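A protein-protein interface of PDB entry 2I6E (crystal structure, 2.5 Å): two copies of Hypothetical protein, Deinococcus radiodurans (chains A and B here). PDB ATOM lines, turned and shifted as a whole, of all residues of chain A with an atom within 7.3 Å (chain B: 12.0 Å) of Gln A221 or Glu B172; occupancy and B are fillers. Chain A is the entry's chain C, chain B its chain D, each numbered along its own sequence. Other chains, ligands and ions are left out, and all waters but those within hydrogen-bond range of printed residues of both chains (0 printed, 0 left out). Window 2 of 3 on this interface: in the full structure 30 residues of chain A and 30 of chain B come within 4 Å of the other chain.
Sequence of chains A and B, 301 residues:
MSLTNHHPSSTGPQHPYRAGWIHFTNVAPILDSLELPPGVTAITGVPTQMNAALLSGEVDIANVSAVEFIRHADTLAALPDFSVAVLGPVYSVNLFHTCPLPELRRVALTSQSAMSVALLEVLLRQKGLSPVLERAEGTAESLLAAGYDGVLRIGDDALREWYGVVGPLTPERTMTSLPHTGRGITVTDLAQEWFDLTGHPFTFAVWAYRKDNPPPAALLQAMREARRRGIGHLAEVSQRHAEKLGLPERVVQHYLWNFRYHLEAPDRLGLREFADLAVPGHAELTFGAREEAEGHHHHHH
NH2 of Arg B250 lies close to NH2 of Arg A228, at 3.2 Å. The guanidinium group (NH1) of Arg A224 lies within hydrogen-bond range of the backbone carbonyl oxygen (O) of Glu B172 (2.8 Å).
O of Arg B173 is in hydrogen-bond range of NH2 of Arg B250 (3.3 Å). The side-chain carboxylate of Asp A81 is in salt-bridge range of the guanidinium group of Arg A227. The side-chain hydroxyl (OG1) of Thr B170 is in hydrogen-bond range of the side-chain carboxylate (OE1) of Glu B172 (2.6 Å). The side-chain hydroxyl of Thr B174 lies close to the backbone NH of Thr B176, at 3.4 Å. The backbone carbonyl oxygen (O) of Thr B170 is in hydrogen-bond range of the guanidinium group (NH1) of Arg B250, 3.0 Å away. NE2 of Gln A221 sits at hydrogen-bond distance from OE1 of Glu A225.
Thr B174 touches Asp A81 (CG2 to OD2, 3.8 Å). CG of Gln A221 touches O of Pro B171, at 3.8 Å. Glu B172 touches Gln A221.
Of the printed residues of chain B, Asp A81 touches Thr B174 (3.8 Å). No residue of chain B comes within 4 Å of Ala A217. No residue of chain B comes within 4 Å of Leu A219. No residue of chain B comes within 4 Å of Leu A220. Of the printed residues of chain B, Gln A221 touches Pro B171 and Glu B172. No residue of chain B comes within 4 Å of Ala A222. Arg A224 touches just one residue of chain B: Glu B172. No residue of chain B comes within 4 Å of Glu A225. Printed residues of chain B within 4 Å of Arg A228: Arg B250 (3.2 Å). Printed residues of chain A within 4 Å of Pro B171: Gln A221. Of the printed residues of chain A, Thr B174 touches Asp A81. Of the printed residues of chain A, Arg B250 touches Arg A228.
Of the 18 printed residues of chain A, 4 touch a printed residue of chain B. Printed residues of chain A that touch a printed residue of chain B: Asp A81, Gln A221, Arg A224 and Arg A228. Printed residues of chain B that touch a printed residue of chain A: Pro B171, Glu B172, Thr B174 and Arg B250. Among the printed residues, 5 pairs touch across the chains.
No position is printed for both chains. Of the 5 pairs that touch across the chains among the printed residues, none has its exchanged pair printed and touching as well.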
ATOM      1  N   LEU A  34       2.814  -3.735 -40.880  1.00  0.00           N
ATOM      2  CA  LEU A  34       3.512  -3.612 -39.604  1.00  0.00           C
ATOM      3  C   LEU A  34       4.848  -2.895 -39.742  1.00  0.00           C
ATOM      4  O   LEU A  34       5.678  -3.254 -40.577  1.00  0.00           O
ATOM      5  CB  LEU A  34       3.749  -4.995 -38.992  1.00  0.00           C
ATOM      6  CG  LEU A  34       4.505  -5.065 -37.658  1.00  0.00           C
ATOM      7  CD1 LEU A  34       3.725  -4.336 -36.582  1.00  0.00           C
ATOM      8  CD2 LEU A  34       4.717  -6.527 -37.260  1.00  0.00           C
ATOM      9  N   GLU A  35       5.043  -1.873 -38.918  1.00  0.00           N
ATOM     10  CA  GLU A  35       6.288  -1.114 -38.907  1.00  0.00           C
ATOM     11  C   GLU A  35       6.986  -1.507 -37.618  1.00  0.00           C
ATOM     12  O   GLU A  35       6.531  -1.160 -36.528  1.00  0.00           O
ATOM     13  CB  GLU A  35       6.007   0.388 -38.895  1.00  0.00           C
ATOM     14  CG  GLU A  35       5.478   0.944 -40.211  1.00  0.00           C
ATOM     15  CD  GLU A  35       4.949   2.364 -40.055  1.00  0.00           C
ATOM     16  OE1 GLU A  35       4.841   3.090 -41.071  1.00  0.00           O
ATOM     17  OE2 GLU A  35       4.632   2.748 -38.910  1.00  0.00           O
ATOM     18  N   PRO A  37       9.221  -1.552 -34.432  1.00  0.00           N
ATOM     19  CA  PRO A  37       9.786  -0.479 -33.609  1.00  0.00           C
ATOM     20  C   PRO A  37      11.303  -0.622 -33.676  1.00  0.00           C
ATOM     21  O   PRO A  37      11.820  -1.639 -34.148  1.00  0.00           O
ATOM     22  CB  PRO A  37       9.255  -0.795 -32.212  1.00  0.00           C
ATOM     23  CG  PRO A  37       7.950  -1.460 -32.489  1.00  0.00           C
ATOM     24  CD  PRO A  37       8.286  -2.376 -33.652  1.00  0.00           C
ATOM     25  N   ASP A  81      -4.873 -10.316 -27.067  1.00  0.00           N
ATOM     26  CA  ASP A  81      -5.849  -9.831 -28.037  1.00  0.00           C
ATOM     27  C   ASP A  81      -5.525 -10.068 -29.507  1.00  0.00           C
ATOM     28  O   ASP A  81      -5.913  -9.266 -30.365  1.00  0.00           O
ATOM     29  CB  ASP A  81      -6.042  -8.342 -27.816  1.00  0.00           C
ATOM     30  CG  ASP A  81      -4.775  -7.562 -28.095  1.00  0.00           C
ATOM     31  OD1 ASP A  81      -3.677  -8.089 -27.802  1.00  0.00           O
ATOM     32  OD2 ASP A  81      -4.874  -6.426 -28.598  1.00  0.00           O
ATOM     33  N   PHE A  82      -4.821 -11.158 -29.797  1.00  0.00           N
ATOM     34  CA  PHE A  82      -4.456 -11.481 -31.171  1.00  0.00           C
ATOM     35  C   PHE A  82      -4.723 -12.935 -31.483  1.00  0.00           C
ATOM     36  O   PHE A  82      -4.216 -13.833 -30.813  1.00  0.00           O
ATOM     37  CB  PHE A  82      -2.985 -11.154 -31.417  1.00  0.00           C
ATOM     38  CG  PHE A  82      -2.751  -9.715 -31.777  1.00  0.00           C
ATOM     39  CD1 PHE A  82      -2.806  -9.301 -33.105  1.00  0.00           C
ATOM     40  CD2 PHE A  82      -2.512  -8.764 -30.785  1.00  0.00           C
ATOM     41  CE1 PHE A  82      -2.627  -7.966 -33.445  1.00  0.00           C
ATOM     42  CE2 PHE A  82      -2.332  -7.422 -31.114  1.00  0.00           C
ATOM     43  CZ  PHE A  82      -2.391  -7.025 -32.445  1.00  0.00           C
ATOM     44  N   PRO A 216       8.096  -6.200 -26.059  1.00  0.00           N
ATOM     45  CA  PRO A 216       8.108  -4.776 -25.716  1.00  0.00           C
ATOM     46  C   PRO A 216       6.807  -4.079 -26.126  1.00  0.00           C
ATOM     47  O   PRO A 216       6.294  -4.291 -27.229  1.00  0.00           O
ATOM     48  CB  PRO A 216       9.321  -4.251 -26.476  1.00  0.00           C
ATOM     49  CG  PRO A 216       9.354  -5.121 -27.686  1.00  0.00           C
ATOM     50  CD  PRO A 216       9.062  -6.494 -27.133  1.00  0.00           C
ATOM     51  N   ALA A 217       6.282  -3.247 -25.232  1.00  0.00           N
ATOM     52  CA  ALA A 217       5.045  -2.519 -25.477  1.00  0.00           C
ATOM     53  C   ALA A 217       4.993  -1.835 -26.842  1.00  0.00           C
ATOM     54  O   ALA A 217       3.924  -1.738 -27.449  1.00  0.00           O
ATOM     55  CB  ALA A 217       4.827  -1.487 -24.375  1.00  0.00           C
ATOM     56  N   ALA A 218       6.135  -1.358 -27.323  1.00  0.00           N
ATOM     57  CA  ALA A 218       6.178  -0.680 -28.615  1.00  0.00           C
ATOM     58  C   ALA A 218       5.813  -1.610 -29.772  1.00  0.00           C
ATOM     59  O   ALA A 218       5.273  -1.167 -30.795  1.00  0.00           O
ATOM     60  CB  ALA A 218       7.561  -0.074 -28.846  1.00  0.00           C
ATOM     61  N   LEU A 219       6.117  -2.895 -29.616  1.00  0.00           N
ATOM     62  CA  LEU A 219       5.795  -3.858 -30.657  1.00  0.00           C
ATOM     63  C   LEU A 219       4.299  -4.123 -30.632  1.00  0.00           C
ATOM     64  O   LEU A 219       3.644  -4.190 -31.671  1.00  0.00           O
ATOM     65  CB  LEU A 219       6.549  -5.172 -30.440  1.00  0.00           C
ATOM     66  CG  LEU A 219       6.261  -6.220 -31.523  1.00  0.00           C
ATOM     67  CD1 LEU A 219       6.655  -5.660 -32.889  1.00  0.00           C
ATOM     68  CD2 LEU A 219       7.021  -7.506 -31.218  1.00  0.00           C
ATOM     69  N   LEU A 220       3.757  -4.275 -29.432  1.00  0.00           N
ATOM     70  CA  LEU A 220       2.340  -4.522 -29.304  1.00  0.00           C
ATOM     71  C   LEU A 220       1.585  -3.354 -29.928  1.00  0.00           C
ATOM     72  O   LEU A 220       0.697  -3.551 -30.757  1.00  0.00           O
ATOM     73  CB  LEU A 220       1.970  -4.697 -27.834  1.00  0.00           C
ATOM     74  CG  LEU A 220       2.740  -5.849 -27.179  1.00  0.00           C
ATOM     75  CD1 LEU A 220       2.321  -6.006 -25.726  1.00  0.00           C
ATOM     76  CD2 LEU A 220       2.481  -7.137 -27.948  1.00  0.00           C
ATOM     77  N   GLN A 221       1.957  -2.136 -29.555  1.00  0.00           N
ATOM     78  CA  GLN A 221       1.294  -0.961 -30.098  1.00  0.00           C
ATOM     79  C   GLN A 221       1.431  -0.927 -31.623  1.00  0.00           C
ATOM     80  O   GLN A 221       0.480  -0.606 -32.334  1.00  0.00           O
ATOM     81  CB  GLN A 221       1.882   0.316 -29.498  1.00  0.00           C
ATOM     82  CG  GLN A 221       1.053   1.548 -29.809  1.00  0.00           C
ATOM     83  CD  GLN A 221       1.617   2.823 -29.211  1.00  0.00           C
ATOM     84  OE1 GLN A 221       1.885   2.903 -28.007  1.00  0.00           O
ATOM     85  NE2 GLN A 221       1.788   3.838 -30.053  1.00  0.00           N
ATOM     86  N   ALA A 222       2.613  -1.256 -32.127  1.00  0.00           N
ATOM     87  CA  ALA A 222       2.820  -1.252 -33.563  1.00  0.00           C
ATOM     88  C   ALA A 222       1.880  -2.278 -34.185  1.00  0.00           C
ATOM     89  O   ALA A 222       1.296  -2.041 -35.244  1.00  0.00           O
ATOM     90  CB  ALA A 222       4.275  -1.592 -33.893  1.00  0.00           C
ATOM     91  N   MET A 223       1.725  -3.415 -33.517  1.00  0.00           N
ATOM     92  CA  MET A 223       0.850  -4.464 -34.017  1.00  0.00           C
ATOM     93  C   MET A 223      -0.620  -4.079 -33.978  1.00  0.00           C
ATOM     94  O   MET A 223      -1.351  -4.313 -34.937  1.00  0.00           O
ATOM     95  CB  MET A 223       1.069  -5.754 -33.231  1.00  0.00           C
ATOM     96  CG  MET A 223       2.325  -6.492 -33.644  1.00  0.00           C
ATOM     97  SD  MET A 223       2.693  -8.046 -32.573  1.00  0.00           S
ATOM     98  CE  MET A 223       1.399  -9.266 -33.339  1.00  0.00           C
ATOM     99  N   ARG A 224      -1.053  -3.484 -32.874  1.00  0.00           N
ATOM    100  CA  ARG A 224      -2.441  -3.073 -32.741  1.00  0.00           C
ATOM    101  C   ARG A 224      -2.744  -2.057 -33.831  1.00  0.00           C
ATOM    102  O   ARG A 224      -3.818  -2.067 -34.427  1.00  0.00           O
ATOM    103  CB  ARG A 224      -2.685  -2.455 -31.363  1.00  0.00           C
ATOM    104  CG  ARG A 224      -2.261  -3.355 -30.207  1.00  0.00           C
ATOM    105  CD  ARG A 224      -3.429  -3.713 -29.303  1.00  0.00           C
ATOM    106  NE  ARG A 224      -3.104  -4.799 -28.373  1.00  0.00           N
ATOM    107  CZ  ARG A 224      -2.304  -4.684 -27.315  1.00  0.00           C
ATOM    108  NH1 ARG A 224      -1.736  -3.516 -27.026  1.00  0.00           N
ATOM    109  NH2 ARG A 224      -2.060  -5.746 -26.555  1.00  0.00           N
ATOM    110  N   GLU A 225      -1.782  -1.184 -34.099  1.00  0.00           N
ATOM    111  CA  GLU A 225      -1.941  -0.157 -35.117  1.00  0.00           C
ATOM    112  C   GLU A 225      -1.972  -0.735 -36.527  1.00  0.00           C
ATOM    113  O   GLU A 225      -2.742  -0.270 -37.380  1.00  0.00           O
ATOM    114  CB  GLU A 225      -0.818   0.880 -35.002  1.00  0.00           C
ATOM    115  CG  GLU A 225      -0.927   1.771 -33.767  1.00  0.00           C
ATOM    116  CD  GLU A 225       0.341   2.557 -33.489  1.00  0.00           C
ATOM    117  OE1 GLU A 225       0.365   3.304 -32.489  1.00  0.00           O
ATOM    118  OE2 GLU A 225       1.312   2.422 -34.265  1.00  0.00           O
ATOM    119  N   ALA A 226      -1.143  -1.745 -36.775  1.00  0.00           N
ATOM    120  CA  ALA A 226      -1.094  -2.358 -38.098  1.00  0.00           C
ATOM    121  C   ALA A 226      -2.411  -3.077 -38.428  1.00  0.00           C
ATOM    122  O   ALA A 226      -2.918  -2.973 -39.545  1.00  0.00           O
ATOM    123  CB  ALA A 226       0.092  -3.324 -38.192  1.00  0.00           C
ATOM    124  N   ARG A 227      -2.964  -3.796 -37.456  1.00  0.00           N
ATOM    125  CA  ARG A 227      -4.227  -4.511 -37.654  1.00  0.00           C
ATOM    126  C   ARG A 227      -5.320  -3.494 -37.985  1.00  0.00           C
ATOM    127  O   ARG A 227      -6.165  -3.712 -38.861  1.00  0.00           O
ATOM    128  CB  ARG A 227      -4.598  -5.296 -36.384  1.00  0.00           C
ATOM    129  CG  ARG A 227      -5.977  -5.941 -36.402  1.00  0.00           C
ATOM    130  CD  ARG A 227      -6.162  -6.868 -35.211  1.00  0.00           C
ATOM    131  NE  ARG A 227      -6.049  -6.143 -33.948  1.00  0.00           N
ATOM    132  CZ  ARG A 227      -5.981  -6.721 -32.754  1.00  0.00           C
ATOM    133  NH1 ARG A 227      -6.011  -8.044 -32.657  1.00  0.00           N
ATOM    134  NH2 ARG A 227      -5.893  -5.973 -31.659  1.00  0.00           N
ATOM    135  N   ARG A 228      -5.283  -2.373 -37.281  1.00  0.00           N
ATOM    136  CA  ARG A 228      -6.251  -1.304 -37.482  1.00  0.00           C
ATOM    137  C   ARG A 228      -6.243  -0.848 -38.950  1.00  0.00           C
ATOM    138  O   ARG A 228      -7.293  -0.634 -39.554  1.00  0.00           O
ATOM    139  CB  ARG A 228      -5.907  -0.153 -36.544  1.00  0.00           C
ATOM    140  CG  ARG A 228      -7.098   0.535 -35.924  1.00  0.00           C
ATOM    141  CD  ARG A 228      -6.650   1.398 -34.753  1.00  0.00           C
ATOM    142  NE  ARG A 228      -6.368   0.616 -33.546  1.00  0.00           N
ATOM    143  CZ  ARG A 228      -5.386   0.889 -32.687  1.00  0.00           C
ATOM    144  NH1 ARG A 228      -4.575   1.919 -32.904  1.00  0.00           N
ATOM    145  NH2 ARG A 228      -5.223   0.147 -31.598  1.00  0.00           N
ATOM    146  N   TYR B 163     -19.185   4.865 -24.330  1.00  0.00           N
ATOM    147  CA  TYR B 163     -17.834   5.385 -24.461  1.00  0.00           C
ATOM    148  C   TYR B 163     -17.606   6.536 -23.489  1.00  0.00           C
ATOM    149  O   TYR B 163     -16.540   6.642 -22.888  1.00  0.00           O
ATOM    150  CB  TYR B 163     -17.581   5.866 -25.893  1.00  0.00           C
ATOM    151  CG  TYR B 163     -16.137   6.236 -26.137  1.00  0.00           C
ATOM    152  CD1 TYR B 163     -15.138   5.266 -26.088  1.00  0.00           C
ATOM    153  CD2 TYR B 163     -15.759   7.558 -26.383  1.00  0.00           C
ATOM    154  CE1 TYR B 163     -13.805   5.597 -26.270  1.00  0.00           C
ATOM    155  CE2 TYR B 163     -14.417   7.900 -26.570  1.00  0.00           C
ATOM    156  CZ  TYR B 163     -13.447   6.909 -26.510  1.00  0.00           C
ATOM    157  OH  TYR B 163     -12.113   7.220 -26.672  1.00  0.00           O
ATOM    158  N   VAL B 166     -17.000   4.474 -20.023  1.00  0.00           N
ATOM    159  CA  VAL B 166     -15.801   3.646 -19.913  1.00  0.00           C
ATOM    160  C   VAL B 166     -14.559   4.164 -20.631  1.00  0.00           C
ATOM    161  O   VAL B 166     -13.479   3.590 -20.487  1.00  0.00           O
ATOM    162  CB  VAL B 166     -16.058   2.212 -20.418  1.00  0.00           C
ATOM    163  CG1 VAL B 166     -17.223   1.594 -19.672  1.00  0.00           C
ATOM    164  CG2 VAL B 166     -16.328   2.232 -21.909  1.00  0.00           C
ATOM    165  N   GLY B 167     -14.705   5.236 -21.401  1.00  0.00           N
ATOM    166  CA  GLY B 167     -13.561   5.778 -22.116  1.00  0.00           C
ATOM    167  C   GLY B 167     -12.680   6.648 -21.234  1.00  0.00           C
ATOM    168  O   GLY B 167     -12.883   6.696 -20.017  1.00  0.00           O
ATOM    169  N   PRO B 168     -11.681   7.342 -21.816  1.00  0.00           N
ATOM    170  CA  PRO B 168     -11.380   7.324 -23.250  1.00  0.00           C
ATOM    171  C   PRO B 168     -10.470   6.164 -23.612  1.00  0.00           C
ATOM    172  O   PRO B 168     -10.035   5.394 -22.754  1.00  0.00           O
ATOM    173  CB  PRO B 168     -10.705   8.666 -23.476  1.00  0.00           C
ATOM    174  CG  PRO B 168      -9.902   8.807 -22.238  1.00  0.00           C
ATOM    175  CD  PRO B 168     -10.875   8.374 -21.139  1.00  0.00           C
ATOM    176  N   LEU B 169     -10.180   6.053 -24.897  1.00  0.00           N
ATOM    177  CA  LEU B 169      -9.333   4.987 -25.387  1.00  0.00           C
ATOM    178  C   LEU B 169      -7.925   5.537 -25.602  1.00  0.00           C
ATOM    179  O   LEU B 169      -7.757   6.661 -26.074  1.00  0.00           O
ATOM    180  CB  LEU B 169      -9.918   4.453 -26.694  1.00  0.00           C
ATOM    181  CG  LEU B 169      -9.531   3.066 -27.199  1.00  0.00           C
ATOM    182  CD1 LEU B 169      -9.561   2.034 -26.074  1.00  0.00           C
ATOM    183  CD2 LEU B 169     -10.507   2.684 -28.297  1.00  0.00           C
ATOM    184  N   THR B 170      -6.920   4.752 -25.226  1.00  0.00           N
ATOM    185  CA  THR B 170      -5.521   5.147 -25.389  1.00  0.00           C
ATOM    186  C   THR B 170      -4.924   4.353 -26.558  1.00  0.00           C
ATOM    187  O   THR B 170      -5.385   3.255 -26.872  1.00  0.00           O
ATOM    188  CB  THR B 170      -4.701   4.855 -24.103  1.00  0.00           C
ATOM    189  OG1 THR B 170      -4.651   3.440 -23.866  1.00  0.00           O
ATOM    190  CG2 THR B 170      -5.339   5.536 -22.900  1.00  0.00           C
ATOM    191  N   PRO B 171      -3.890   4.899 -27.218  1.00  0.00           N
ATOM    192  CA  PRO B 171      -3.255   4.214 -28.349  1.00  0.00           C
ATOM    193  C   PRO B 171      -2.655   2.835 -28.058  1.00  0.00           C
ATOM    194  O   PRO B 171      -2.616   1.978 -28.945  1.00  0.00           O
ATOM    195  CB  PRO B 171      -2.208   5.223 -28.815  1.00  0.00           C
ATOM    196  CG  PRO B 171      -1.874   5.973 -27.562  1.00  0.00           C
ATOM    197  CD  PRO B 171      -3.240   6.195 -26.963  1.00  0.00           C
ATOM    198  N   GLU B 172      -2.193   2.611 -26.828  1.00  0.00           N
ATOM    199  CA  GLU B 172      -1.607   1.314 -26.486  1.00  0.00           C
ATOM    200  C   GLU B 172      -2.675   0.269 -26.169  1.00  0.00           C
ATOM    201  O   GLU B 172      -2.545  -0.896 -26.544  1.00  0.00           O
ATOM    202  CB  GLU B 172      -0.648   1.428 -25.288  1.00  0.00           C
ATOM    203  CG  GLU B 172      -1.318   1.656 -23.936  1.00  0.00           C
ATOM    204  CD  GLU B 172      -1.741   3.098 -23.732  1.00  0.00           C
ATOM    205  OE1 GLU B 172      -2.361   3.395 -22.688  1.00  0.00           O
ATOM    206  OE2 GLU B 172      -1.446   3.936 -24.616  1.00  0.00           O
ATOM    207  N   ARG B 173      -3.729   0.696 -25.480  1.00  0.00           N
ATOM    208  CA  ARG B 173      -4.815  -0.201 -25.103  1.00  0.00           C
ATOM    209  C   ARG B 173      -5.799  -0.383 -26.258  1.00  0.00           C
ATOM    210  O   ARG B 173      -5.916   0.475 -27.130  1.00  0.00           O
ATOM    211  CB  ARG B 173      -5.527   0.358 -23.863  1.00  0.00           C
ATOM    212  CG  ARG B 173      -6.194  -0.688 -22.959  1.00  0.00           C
ATOM    213  CD  ARG B 173      -5.271  -1.883 -22.647  1.00  0.00           C
ATOM    214  NE  ARG B 173      -3.930  -1.507 -22.184  1.00  0.00           N
ATOM    215  CZ  ARG B 173      -3.659  -0.922 -21.019  1.00  0.00           C
ATOM    216  NH1 ARG B 173      -4.639  -0.630 -20.171  1.00  0.00           N
ATOM    217  NH2 ARG B 173      -2.401  -0.632 -20.697  1.00  0.00           N
ATOM    218  N   THR B 174      -6.494  -1.516 -26.267  1.00  0.00           N
ATOM    219  CA  THR B 174      -7.467  -1.817 -27.313  1.00  0.00           C
ATOM    220  C   THR B 174      -8.891  -1.614 -26.791  1.00  0.00           C
ATOM    221  O   THR B 174      -9.125  -1.638 -25.582  1.00  0.00           O
ATOM    222  CB  THR B 174      -7.300  -3.276 -27.813  1.00  0.00           C
ATOM    223  OG1 THR B 174      -8.347  -3.597 -28.738  1.00  0.00           O
ATOM    224  CG2 THR B 174      -7.335  -4.250 -26.639  1.00  0.00           C
ATOM    225  N   MET B 175      -9.836  -1.401 -27.703  1.00  0.00           N
ATOM    226  CA  MET B 175     -11.230  -1.194 -27.317  1.00  0.00           C
ATOM    227  C   MET B 175     -11.758  -2.443 -26.625  1.00  0.00           C
ATOM    228  O   MET B 175     -12.475  -2.367 -25.625  1.00  0.00           O
ATOM    229  CB  MET B 175     -12.091  -0.886 -28.548  1.00  0.00           C
ATOM    230  CG  MET B 175     -13.532  -0.499 -28.225  1.00  0.00           C
ATOM    231  SD  MET B 175     -14.550   0.110 -29.771  1.00  0.00           S
ATOM    232  CE  MET B 175     -16.224  -0.829 -29.517  1.00  0.00           C
ATOM    233  N   THR B 176     -11.382  -3.595 -27.164  1.00  0.00           N
ATOM    234  CA  THR B 176     -11.806  -4.887 -26.639  1.00  0.00           C
ATOM    235  C   THR B 176     -11.289  -5.158 -25.217  1.00  0.00           C
ATOM    236  O   THR B 176     -11.577  -6.200 -24.635  1.00  0.00           O
ATOM    237  CB  THR B 176     -11.336  -6.021 -27.580  1.00  0.00           C
ATOM    238  OG1 THR B 176     -12.020  -7.233 -27.250  1.00  0.00           O
ATOM    239  CG2 THR B 176      -9.837  -6.240 -27.456  1.00  0.00           C
ATOM    240  N   SER B 177     -10.532  -4.217 -24.661  1.00  0.00           N
ATOM    241  CA  SER B 177      -9.981  -4.372 -23.319  1.00  0.00           C
ATOM    242  C   SER B 177     -10.318  -3.147 -22.489  1.00  0.00           C
ATOM    243  O   SER B 177      -9.650  -2.840 -21.502  1.00  0.00           O
ATOM    244  CB  SER B 177      -8.460  -4.528 -23.382  1.00  0.00           C
ATOM    245  OG  SER B 177      -7.833  -3.299 -23.712  1.00  0.00           O
ATOM    246  N   LEU B 178     -11.356  -2.440 -22.913  1.00  0.00           N
ATOM    247  CA  LEU B 178     -11.805  -1.237 -22.230  1.00  0.00           C
ATOM    248  C   LEU B 178     -12.627  -1.699 -21.021  1.00  0.00           C
ATOM    249  O   LEU B 178     -13.274  -2.747 -21.068  1.00  0.00           O
ATOM    250  CB  LEU B 178     -12.641  -0.403 -23.209  1.00  0.00           C
ATOM    251  CG  LEU B 178     -12.634   1.129 -23.193  1.00  0.00           C
ATOM    252  CD1 LEU B 178     -11.255   1.687 -22.924  1.00  0.00           C
ATOM    253  CD2 LEU B 178     -13.134   1.611 -24.536  1.00  0.00           C
ATOM    254  N   PRO B 179     -12.599  -0.934 -19.919  1.00  0.00           N
ATOM    255  CA  PRO B 179     -13.341  -1.280 -18.700  1.00  0.00           C
ATOM    256  C   PRO B 179     -14.858  -1.357 -18.872  1.00  0.00           C
ATOM    257  O   PRO B 179     -15.413  -0.876 -19.862  1.00  0.00           O
ATOM    258  CB  PRO B 179     -12.934  -0.181 -17.726  1.00  0.00           C
ATOM    259  CG  PRO B 179     -12.730   0.993 -18.629  1.00  0.00           C
ATOM    260  CD  PRO B 179     -11.960   0.385 -19.781  1.00  0.00           C
ATOM    261  N   PRO B 248     -14.063   8.669 -31.614  1.00  0.00           N
ATOM    262  CA  PRO B 248     -12.799   8.445 -32.320  1.00  0.00           C
ATOM    263  C   PRO B 248     -13.072   7.487 -33.486  1.00  0.00           C
ATOM    264  O   PRO B 248     -13.864   6.556 -33.352  1.00  0.00           O
ATOM    265  CB  PRO B 248     -11.911   7.799 -31.255  1.00  0.00           C
ATOM    266  CG  PRO B 248     -12.432   8.363 -29.981  1.00  0.00           C
ATOM    267  CD  PRO B 248     -13.934   8.353 -30.180  1.00  0.00           C
ATOM    268  N   ARG B 250     -11.423   5.060 -34.645  1.00  0.00           N
ATOM    269  CA  ARG B 250     -11.160   3.672 -34.294  1.00  0.00           C
ATOM    270  C   ARG B 250     -12.282   3.022 -33.491  1.00  0.00           C
ATOM    271  O   ARG B 250     -12.402   1.800 -33.483  1.00  0.00           O
ATOM    272  CB  ARG B 250      -9.832   3.543 -33.537  1.00  0.00           C
ATOM    273  CG  ARG B 250      -9.744   4.375 -32.269  1.00  0.00           C
ATOM    274  CD  ARG B 250      -8.495   4.042 -31.483  1.00  0.00           C
ATOM    275  NE  ARG B 250      -8.474   2.640 -31.070  1.00  0.00           N
ATOM    276  CZ  ARG B 250      -7.699   2.155 -30.106  1.00  0.00           C
ATOM    277  NH1 ARG B 250      -6.875   2.962 -29.444  1.00  0.00           N
ATOM    278  NH2 ARG B 250      -7.755   0.865 -29.800  1.00  0.00           N
